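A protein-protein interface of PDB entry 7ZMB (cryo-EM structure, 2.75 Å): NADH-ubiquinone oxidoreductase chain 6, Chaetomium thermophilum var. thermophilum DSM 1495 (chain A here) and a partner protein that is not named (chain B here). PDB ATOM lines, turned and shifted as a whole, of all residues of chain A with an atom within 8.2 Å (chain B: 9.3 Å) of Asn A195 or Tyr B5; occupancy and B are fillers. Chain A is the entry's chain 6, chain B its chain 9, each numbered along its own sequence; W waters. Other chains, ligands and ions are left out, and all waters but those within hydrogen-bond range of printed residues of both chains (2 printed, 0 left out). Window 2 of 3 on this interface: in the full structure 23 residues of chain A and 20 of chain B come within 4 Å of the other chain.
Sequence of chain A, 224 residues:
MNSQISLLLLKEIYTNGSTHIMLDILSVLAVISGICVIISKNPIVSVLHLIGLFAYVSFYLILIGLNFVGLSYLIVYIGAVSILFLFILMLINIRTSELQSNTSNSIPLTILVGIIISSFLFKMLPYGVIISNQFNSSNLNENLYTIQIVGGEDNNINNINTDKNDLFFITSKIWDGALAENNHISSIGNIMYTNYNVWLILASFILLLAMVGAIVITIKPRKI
OG of Ser A187 is in hydrogen-bond range of O of Leu B7. The side-chain hydroxyl (OG) of Ser A187 lies within hydrogen-bond range of the backbone NH (N) of Gly B9, at 3.2 Å. The side-chain amide nitrogen (ND2) of Asn A195 lies within hydrogen-bond range of the side-chain hydroxyl (OH) of Tyr B5, at 2.9 Å.
The backbone carbonyl oxygen of Ile A191 sits at hydrogen-bond distance from the backbone NH of Tyr A196 (3.1 Å). OD1 of Asn A195 is in hydrogen-bond range of OG1 of Thr A194. OG of Ser B3 lies within hydrogen-bond range of N of Tyr B5, at 3.3 Å. The side-chain amide oxygen of Asn B8 lies within hydrogen-bond range of the backbone NH of Gly B10, at 3.1 Å.
Ser A187 touches Asn B8 (OG to C, 3.6 Å). CG2 of Ile A191 touches CD1 of Tyr B5 (3.6 Å). Ser B3 touches Tyr A196. Tyr B5 touches Tyr A196 (CE2 to OH, 3.8 Å).
Of the printed residues of chain B, Ser A187 touches Leu B7, Asn B8 and Gly B9. No residue of chain B comes within 4 Å of Thr A194. Tyr A196 touches two residues of chain B. Trp A199 touches none of the printed residues of chain B. No residue of chain A comes within 4 Å of Gly B4. Tyr B5 touches just these residues of chain A: Ile A191 (3.6 Å), Asn A195 (2.9 Å) and Tyr A196 (3.8 Å). No residue of chain A comes within 4 Å of Gly B6. Of the printed residues of chain A, Asn B8 touches Ser A187. Printed residues of chain A within 4 Å of Gly B9: Ser A187. Arg B13 touches none of the printed residues of chain A.
Of the 13 printed residues of chain A, 4 touch a printed residue of chain B. Printed residues of chain A that touch a printed residue of chain B: Ser A187, Ile A191, Asn A195 and Tyr A196. Of the 16 printed residues of chain B, 5 touch a printed residue of chain A. Among the printed residues, 7 pairs touch across the chains. Among the printed residues, no Asp or Glu carboxylate lies within 4 Å of a Lys or Arg side-chain nitrogen of the other chain.
Water W2 lies within hydrogen-bond range of the side-chain hydroxyl of Tyr B5 (2.7 Å) and the side-chain amide nitrogen of Asn A195 (3.3 Å). Water W1 lies within hydrogen-bond range of the side-chain amide nitrogen of Asn A195 and the side-chain hydroxyl of Tyr B5.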
ATOM      1  N   SER A 187       2.210 -20.837  -3.187  1.00  0.00           N
ATOM      2  CA  SER A 187       3.640 -20.508  -2.965  1.00  0.00           C
ATOM      3  C   SER A 187       4.122 -19.567  -4.061  1.00  0.00           C
ATOM      4  O   SER A 187       4.934 -18.676  -3.769  1.00  0.00           O
ATOM      5  CB  SER A 187       4.490 -21.724  -2.888  1.00  0.00           C
ATOM      6  OG  SER A 187       3.885 -22.694  -2.053  1.00  0.00           O
ATOM      7  N   ILE A 188       3.598 -19.750  -5.265  1.00  0.00           N
ATOM      8  CA  ILE A 188       3.980 -18.879  -6.402  1.00  0.00           C
ATOM      9  C   ILE A 188       3.203 -17.574  -6.213  1.00  0.00           C
ATOM     10  O   ILE A 188       3.824 -16.519  -6.344  1.00  0.00           O
ATOM     11  CB  ILE A 188       3.613 -19.580  -7.720  1.00  0.00           C
ATOM     12  CG1 ILE A 188       4.557 -20.733  -8.059  1.00  0.00           C
ATOM     13  CG2 ILE A 188       3.507 -18.588  -8.870  1.00  0.00           C
ATOM     14  CD1 ILE A 188       4.046 -21.645  -9.143  1.00  0.00           C
ATOM     15  N   GLY A 189       1.925 -17.647  -5.845  1.00  0.00           N
ATOM     16  CA  GLY A 189       1.187 -16.425  -5.590  1.00  0.00           C
ATOM     17  C   GLY A 189       1.776 -15.588  -4.476  1.00  0.00           C
ATOM     18  O   GLY A 189       1.665 -14.362  -4.494  1.00  0.00           O
ATOM     19  N   ASN A 190       2.423 -16.228  -3.502  1.00  0.00           N
ATOM     20  CA  ASN A 190       3.032 -15.492  -2.402  1.00  0.00           C
ATOM     21  C   ASN A 190       4.122 -14.542  -2.872  1.00  0.00           C
ATOM     22  O   ASN A 190       4.478 -13.618  -2.137  1.00  0.00           O
ATOM     23  CB  ASN A 190       3.604 -16.463  -1.372  1.00  0.00           C
ATOM     24  CG  ASN A 190       2.538 -17.078  -0.485  1.00  0.00           C
ATOM     25  OD1 ASN A 190       1.419 -16.581  -0.397  1.00  0.00           O
ATOM     26  ND2 ASN A 190       2.885 -18.172   0.177  1.00  0.00           N
ATOM     27  N   ILE A 191       4.667 -14.748  -4.069  1.00  0.00           N
ATOM     28  CA  ILE A 191       5.794 -13.954  -4.550  1.00  0.00           C
ATOM     29  C   ILE A 191       5.625 -13.446  -5.972  1.00  0.00           C
ATOM     30  O   ILE A 191       6.371 -12.545  -6.392  1.00  0.00           O
ATOM     31  CB  ILE A 191       7.103 -14.765  -4.427  1.00  0.00           C
ATOM     32  CG1 ILE A 191       7.008 -16.011  -5.294  1.00  0.00           C
ATOM     33  CG2 ILE A 191       7.396 -15.130  -2.988  1.00  0.00           C
ATOM     34  CD1 ILE A 191       8.269 -16.717  -5.416  1.00  0.00           C
ATOM     35  N   MET A 192       4.681 -13.959  -6.757  1.00  0.00           N
ATOM     36  CA  MET A 192       4.537 -13.546  -8.147  1.00  0.00           C
ATOM     37  C   MET A 192       4.090 -12.091  -8.278  1.00  0.00           C
ATOM     38  O   MET A 192       4.306 -11.476  -9.326  1.00  0.00           O
ATOM     39  CB  MET A 192       3.562 -14.512  -8.838  1.00  0.00           C
ATOM     40  CG  MET A 192       2.902 -14.031 -10.108  1.00  0.00           C
ATOM     41  SD  MET A 192       1.840 -15.282 -10.840  1.00  0.00           S
ATOM     42  CE  MET A 192       3.011 -16.144 -11.882  1.00  0.00           C
ATOM     43  N   TYR A 193       3.508 -11.520  -7.227  1.00  0.00           N
ATOM     44  CA  TYR A 193       2.957 -10.177  -7.277  1.00  0.00           C
ATOM     45  C   TYR A 193       3.635  -9.193  -6.334  1.00  0.00           C
ATOM     46  O   TYR A 193       3.256  -8.021  -6.313  1.00  0.00           O
ATOM     47  CB  TYR A 193       1.451 -10.212  -6.977  1.00  0.00           C
ATOM     48  CG  TYR A 193       0.692 -11.216  -7.796  1.00  0.00           C
ATOM     49  CD1 TYR A 193       0.201 -10.888  -9.043  1.00  0.00           C
ATOM     50  CD2 TYR A 193       0.482 -12.497  -7.329  1.00  0.00           C
ATOM     51  CE1 TYR A 193      -0.485 -11.802  -9.795  1.00  0.00           C
ATOM     52  CE2 TYR A 193      -0.200 -13.417  -8.072  1.00  0.00           C
ATOM     53  CZ  TYR A 193      -0.687 -13.064  -9.306  1.00  0.00           C
ATOM     54  OH  TYR A 193      -1.372 -13.991 -10.041  1.00  0.00           O
ATOM     55  N   THR A 194       4.711  -9.602  -5.684  1.00  0.00           N
ATOM     56  CA  THR A 194       5.473  -8.650  -4.841  1.00  0.00           C
ATOM     57  C   THR A 194       6.952  -8.769  -5.187  1.00  0.00           C
ATOM     58  O   THR A 194       7.451  -7.863  -5.854  1.00  0.00           O
ATOM     59  CB  THR A 194       5.222  -8.896  -3.347  1.00  0.00           C
ATOM     60  OG1 THR A 194       5.518 -10.256  -3.027  1.00  0.00           O
ATOM     61  CG2 THR A 194       3.808  -8.565  -2.922  1.00  0.00           C
ATOM     62  N   ASN A 195       7.598  -9.861  -4.789  1.00  0.00           N
ATOM     63  CA  ASN A 195       9.065 -10.037  -4.955  1.00  0.00           C
ATOM     64  C   ASN A 195       9.482 -10.044  -6.428  1.00  0.00           C
ATOM     65  O   ASN A 195      10.554  -9.503  -6.725  1.00  0.00           O
ATOM     66  CB  ASN A 195       9.509 -11.308  -4.230  1.00  0.00           C
ATOM     67  CG  ASN A 195       9.096 -11.360  -2.774  1.00  0.00           C
ATOM     68  OD1 ASN A 195       7.965 -11.709  -2.454  1.00  0.00           O
ATOM     69  ND2 ASN A 195      10.014 -11.031  -1.882  1.00  0.00           N
ATOM     70  N   TYR A 196       8.684 -10.652  -7.308  1.00  0.00           N
ATOM     71  CA  TYR A 196       9.075 -10.787  -8.737  1.00  0.00           C
ATOM     72  C   TYR A 196       8.070 -10.078  -9.657  1.00  0.00           C
ATOM     73  O   TYR A 196       7.960 -10.485 -10.814  1.00  0.00           O
ATOM     74  CB  TYR A 196       9.338 -12.263  -9.047  1.00  0.00           C
ATOM     75  CG  TYR A 196      10.365 -12.888  -8.137  1.00  0.00           C
ATOM     76  CD1 TYR A 196      11.719 -12.773  -8.402  1.00  0.00           C
ATOM     77  CD2 TYR A 196       9.986 -13.556  -6.986  1.00  0.00           C
ATOM     78  CE1 TYR A 196      12.668 -13.327  -7.562  1.00  0.00           C
ATOM     79  CE2 TYR A 196      10.923 -14.101  -6.127  1.00  0.00           C
ATOM     80  CZ  TYR A 196      12.270 -13.992  -6.417  1.00  0.00           C
ATOM     81  OH  TYR A 196      13.193 -14.542  -5.577  1.00  0.00           O
ATOM     82  N   ASN A 197       7.426  -9.011  -9.191  1.00  0.00           N
ATOM     83  CA  ASN A 197       6.397  -8.289  -9.991  1.00  0.00           C
ATOM     84  C   ASN A 197       6.953  -7.665 -11.288  1.00  0.00           C
ATOM     85  O   ASN A 197       6.135  -7.333 -12.149  1.00  0.00           O
ATOM     86  CB  ASN A 197       5.491  -7.412  -9.113  1.00  0.00           C
ATOM     87  CG  ASN A 197       6.146  -6.202  -8.491  1.00  0.00           C
ATOM     88  OD1 ASN A 197       7.154  -5.700  -8.978  1.00  0.00           O
ATOM     89  ND2 ASN A 197       5.547  -5.707  -7.423  1.00  0.00           N
ATOM     90  N   VAL A 198       8.262  -7.463 -11.413  1.00  0.00           N
ATOM     91  CA  VAL A 198       8.880  -6.941 -12.664  1.00  0.00           C
ATOM     92  C   VAL A 198       8.627  -7.943 -13.791  1.00  0.00           C
ATOM     93  O   VAL A 198       8.278  -7.519 -14.890  1.00  0.00           O
ATOM     94  CB  VAL A 198      10.379  -6.634 -12.462  1.00  0.00           C
ATOM     95  CG1 VAL A 198      11.236  -6.972 -13.673  1.00  0.00           C
ATOM     96  CG2 VAL A 198      10.610  -5.200 -12.016  1.00  0.00           C
ATOM     97  N   TRP A 199       8.726  -9.228 -13.501  1.00  0.00           N
ATOM     98  CA  TRP A 199       8.501 -10.275 -14.522  1.00  0.00           C
ATOM     99  C   TRP A 199       7.046 -10.230 -14.950  1.00  0.00           C
ATOM    100  O   TRP A 199       6.803 -10.400 -16.135  1.00  0.00           O
ATOM    101  CB  TRP A 199       8.882 -11.668 -14.011  1.00  0.00           C
ATOM    102  CG  TRP A 199      10.323 -11.840 -13.652  1.00  0.00           C
ATOM    103  CD1 TRP A 199      11.377 -11.066 -14.040  1.00  0.00           C
ATOM    104  CD2 TRP A 199      10.874 -12.888 -12.838  1.00  0.00           C
ATOM    105  NE1 TRP A 199      12.542 -11.556 -13.516  1.00  0.00           N
ATOM    106  CE2 TRP A 199      12.267 -12.673 -12.776  1.00  0.00           C
ATOM    107  CE3 TRP A 199      10.326 -13.981 -12.158  1.00  0.00           C
ATOM    108  CZ2 TRP A 199      13.115 -13.511 -12.057  1.00  0.00           C
ATOM    109  CZ3 TRP A 199      11.166 -14.808 -11.451  1.00  0.00           C
ATOM    110  CH2 TRP A 199      12.540 -14.574 -11.403  1.00  0.00           C
ATOM    111  N   MET B   1      17.058 -23.839  -2.955  1.00  0.00           N
ATOM    112  CA  MET B   1      17.976 -23.193  -3.937  1.00  0.00           C
ATOM    113  C   MET B   1      18.323 -21.776  -3.493  1.00  0.00           C
ATOM    114  O   MET B   1      18.050 -21.459  -2.333  1.00  0.00           O
ATOM    115  CB  MET B   1      17.417 -23.202  -5.358  1.00  0.00           C
ATOM    116  N   ALA B   2      18.930 -20.976  -4.363  1.00  0.00           N
ATOM    117  CA  ALA B   2      19.442 -19.638  -3.972  1.00  0.00           C
ATOM    118  C   ALA B   2      18.352 -18.621  -3.613  1.00  0.00           C
ATOM    119  O   ALA B   2      18.698 -17.670  -2.931  1.00  0.00           O
ATOM    120  CB  ALA B   2      20.379 -19.121  -5.024  1.00  0.00           C
ATOM    121  N   SER B   3      17.126 -18.759  -4.114  1.00  0.00           N
ATOM    122  CA  SER B   3      16.061 -17.740  -3.911  1.00  0.00           C
ATOM    123  C   SER B   3      15.600 -17.527  -2.459  1.00  0.00           C
ATOM    124  O   SER B   3      15.477 -16.366  -2.084  1.00  0.00           O
ATOM    125  CB  SER B   3      14.891 -18.046  -4.803  1.00  0.00           C
ATOM    126  OG  SER B   3      14.195 -19.200  -4.359  1.00  0.00           O
ATOM    127  N   GLY B   4      15.277 -18.566  -1.690  1.00  0.00           N
ATOM    128  CA  GLY B   4      14.756 -18.337  -0.331  1.00  0.00           C
ATOM    129  C   GLY B   4      13.296 -18.705  -0.251  1.00  0.00           C
ATOM    130  O   GLY B   4      12.707 -18.562   0.824  1.00  0.00           O
ATOM    131  N   TYR B   5      12.739 -19.178  -1.361  1.00  0.00           N
ATOM    132  CA  TYR B   5      11.290 -19.476  -1.421  1.00  0.00           C
ATOM    133  C   TYR B   5      11.138 -20.906  -1.919  1.00  0.00           C
ATOM    134  O   TYR B   5      11.460 -21.179  -3.081  1.00  0.00           O
ATOM    135  CB  TYR B   5      10.608 -18.432  -2.304  1.00  0.00           C
ATOM    136  CG  TYR B   5      10.844 -17.015  -1.849  1.00  0.00           C
ATOM    137  CD1 TYR B   5      10.055 -16.444  -0.866  1.00  0.00           C
ATOM    138  CD2 TYR B   5      11.882 -16.259  -2.368  1.00  0.00           C
ATOM    139  CE1 TYR B   5      10.279 -15.153  -0.421  1.00  0.00           C
ATOM    140  CE2 TYR B   5      12.125 -14.971  -1.928  1.00  0.00           C
ATOM    141  CZ  TYR B   5      11.317 -14.412  -0.955  1.00  0.00           C
ATOM    142  OH  TYR B   5      11.543 -13.138  -0.522  1.00  0.00           O
ATOM    143  N   GLY B   6      10.667 -21.790  -1.048  1.00  0.00           N
ATOM    144  CA  GLY B   6      10.539 -23.204  -1.412  1.00  0.00           C
ATOM    145  C   GLY B   6       9.149 -23.570  -1.872  1.00  0.00           C
ATOM    146  O   GLY B   6       8.304 -22.670  -1.977  1.00  0.00           O
ATOM    147  N   LEU B   7       8.879 -24.870  -2.000  1.00  0.00           N
ATOM    148  CA  LEU B   7       7.602 -25.364  -2.576  1.00  0.00           C
ATOM    149  C   LEU B   7       6.388 -25.259  -1.640  1.00  0.00           C
ATOM    150  O   LEU B   7       5.278 -25.090  -2.175  1.00  0.00           O
ATOM    151  CB  LEU B   7       7.830 -26.781  -3.106  1.00  0.00           C
ATOM    152  CG  LEU B   7       8.951 -26.905  -4.135  1.00  0.00           C
ATOM    153  CD1 LEU B   7       9.274 -28.358  -4.424  1.00  0.00           C
ATOM    154  CD2 LEU B   7       8.597 -26.168  -5.415  1.00  0.00           C
ATOM    155  N   ASN B   8       6.569 -25.310  -0.320  1.00  0.00           N
ATOM    156  CA  ASN B   8       5.411 -25.281   0.620  1.00  0.00           C
ATOM    157  C   ASN B   8       5.084 -23.868   1.108  1.00  0.00           C
ATOM    158  O   ASN B   8       4.232 -23.752   1.990  1.00  0.00           O
ATOM    159  CB  ASN B   8       5.525 -26.317   1.741  1.00  0.00           C
ATOM    160  CG  ASN B   8       6.527 -26.002   2.836  1.00  0.00           C
ATOM    161  OD1 ASN B   8       6.429 -24.986   3.518  1.00  0.00           O
ATOM    162  ND2 ASN B   8       7.470 -26.901   3.055  1.00  0.00           N
ATOM    163  N   GLY B   9       5.723 -22.844   0.559  1.00  0.00           N
ATOM    164  CA  GLY B   9       5.513 -21.476   1.064  1.00  0.00           C
ATOM    165  C   GLY B   9       6.534 -21.177   2.121  1.00  0.00           C
ATOM    166  O   GLY B   9       6.575 -20.036   2.576  1.00  0.00           O
ATOM    167  N   GLY B  10       7.284 -22.197   2.538  1.00  0.00           N
ATOM    168  CA  GLY B  10       8.390 -21.992   3.480  1.00  0.00           C
ATOM    169  C   GLY B  10       9.681 -21.742   2.724  1.00  0.00           C
ATOM    170  O   GLY B  10       9.645 -21.608   1.504  1.00  0.00           O
ATOM    171  N   PRO B  11      10.858 -21.639   3.390  1.00  0.00           N
ATOM    172  CA  PRO B  11      12.112 -21.282   2.704  1.00  0.00           C
ATOM    173  C   PRO B  11      12.839 -22.425   1.981  1.00  0.00           C
ATOM    174  O   PRO B  11      12.674 -23.552   2.361  1.00  0.00           O
ATOM    175  CB  PRO B  11      13.001 -20.755   3.828  1.00  0.00           C
ATOM    176  CG  PRO B  11      12.128 -20.679   5.053  1.00  0.00           C
ATOM    177  CD  PRO B  11      11.106 -21.764   4.840  1.00  0.00           C
ATOM    178  N   SER B  12      13.600 -22.111   0.940  1.00  0.00           N
ATOM    179  CA  SER B  12      14.298 -23.152   0.141  1.00  0.00           C
ATOM    180  C   SER B  12      15.343 -23.906   0.987  1.00  0.00           C
ATOM    181  O   SER B  12      16.047 -23.250   1.753  1.00  0.00           O
ATOM    182  CB  SER B  12      14.847 -22.548  -1.129  1.00  0.00           C
ATOM    183  OG  SER B  12      15.797 -21.538  -0.853  1.00  0.00           O
ATOM    184  N   ARG B  13      15.446 -25.230   0.847  1.00  0.00           N
ATOM    185  CA  ARG B  13      16.352 -26.033   1.719  1.00  0.00           C
ATOM    186  C   ARG B  13      17.835 -25.700   1.526  1.00  0.00           C
ATOM    187  O   ARG B  13      18.594 -25.976   2.451  1.00  0.00           O
ATOM    188  CB  ARG B  13      16.163 -27.528   1.439  1.00  0.00           C
ATOM    189  CG  ARG B  13      16.302 -27.925  -0.018  1.00  0.00           C
ATOM    190  CD  ARG B  13      16.217 -29.425  -0.195  1.00  0.00           C
ATOM    191  NE  ARG B  13      16.724 -29.767  -1.511  1.00  0.00           N
ATOM    192  CZ  ARG B  13      17.992 -30.054  -1.754  1.00  0.00           C
ATOM    193  NH1 ARG B  13      18.384 -30.342  -2.982  1.00  0.00           N
ATOM    194  NH2 ARG B  13      18.861 -30.054  -0.764  1.00  0.00           N
ATOM    195  N   CYS B  14      18.227 -25.141   0.387  1.00  0.00           N
ATOM    196  CA  CYS B  14      19.619 -24.775   0.155  1.00  0.00           C
ATOM    197  C   CYS B  14      19.875 -23.294   0.367  1.00  0.00           C
ATOM    198  O   CYS B  14      20.965 -22.814   0.053  1.00  0.00           O
ATOM    199  CB  CYS B  14      20.062 -25.179  -1.254  1.00  0.00           C
ATOM    200  SG  CYS B  14      20.312 -26.941  -1.482  1.00  0.00           S
ATOM    201  N   PHE B  15      18.896 -22.561   0.885  1.00  0.00           N
ATOM    202  CA  PHE B  15      19.102 -21.145   1.153  1.00  0.00           C
ATOM    203  C   PHE B  15      20.146 -20.864   2.230  1.00  0.00           C
ATOM    204  O   PHE B  15      20.941 -19.930   2.038  1.00  0.00           O
ATOM    205  CB  PHE B  15      17.766 -20.480   1.488  1.00  0.00           C
ATOM    206  CG  PHE B  15      17.817 -18.994   1.414  1.00  0.00           C
ATOM    207  CD1 PHE B  15      18.220 -18.369   0.251  1.00  0.00           C
ATOM    208  CD2 PHE B  15      17.488 -18.221   2.506  1.00  0.00           C
ATOM    209  CE1 PHE B  15      18.284 -17.009   0.181  1.00  0.00           C
ATOM    210  CE2 PHE B  15      17.549 -16.855   2.435  1.00  0.00           C
ATOM    211  CZ  PHE B  15      17.940 -16.248   1.273  1.00  0.00           C
ATOM    212  N   PRO B  16      20.192 -21.577   3.367  1.00  0.00           N
ATOM    213  CA  PRO B  16      21.258 -21.297   4.340  1.00  0.00           C
ATOM    214  C   PRO B  16      22.652 -21.476   3.772  1.00  0.00           C
ATOM    215  O   PRO B  16      23.569 -20.725   4.115  1.00  0.00           O
ATOM    216  CB  PRO B  16      20.968 -22.300   5.463  1.00  0.00           C
ATOM    217  CG  PRO B  16      19.541 -22.583   5.343  1.00  0.00           C
ATOM    218  CD  PRO B  16      19.280 -22.611   3.879  1.00  0.00           C
HETATM  219  O   HOH W   1      12.348 -11.879  -3.312  1.00  0.00           O
HETATM  220  O   HOH W   2       9.648 -12.164   1.215  1.00  0.00           O
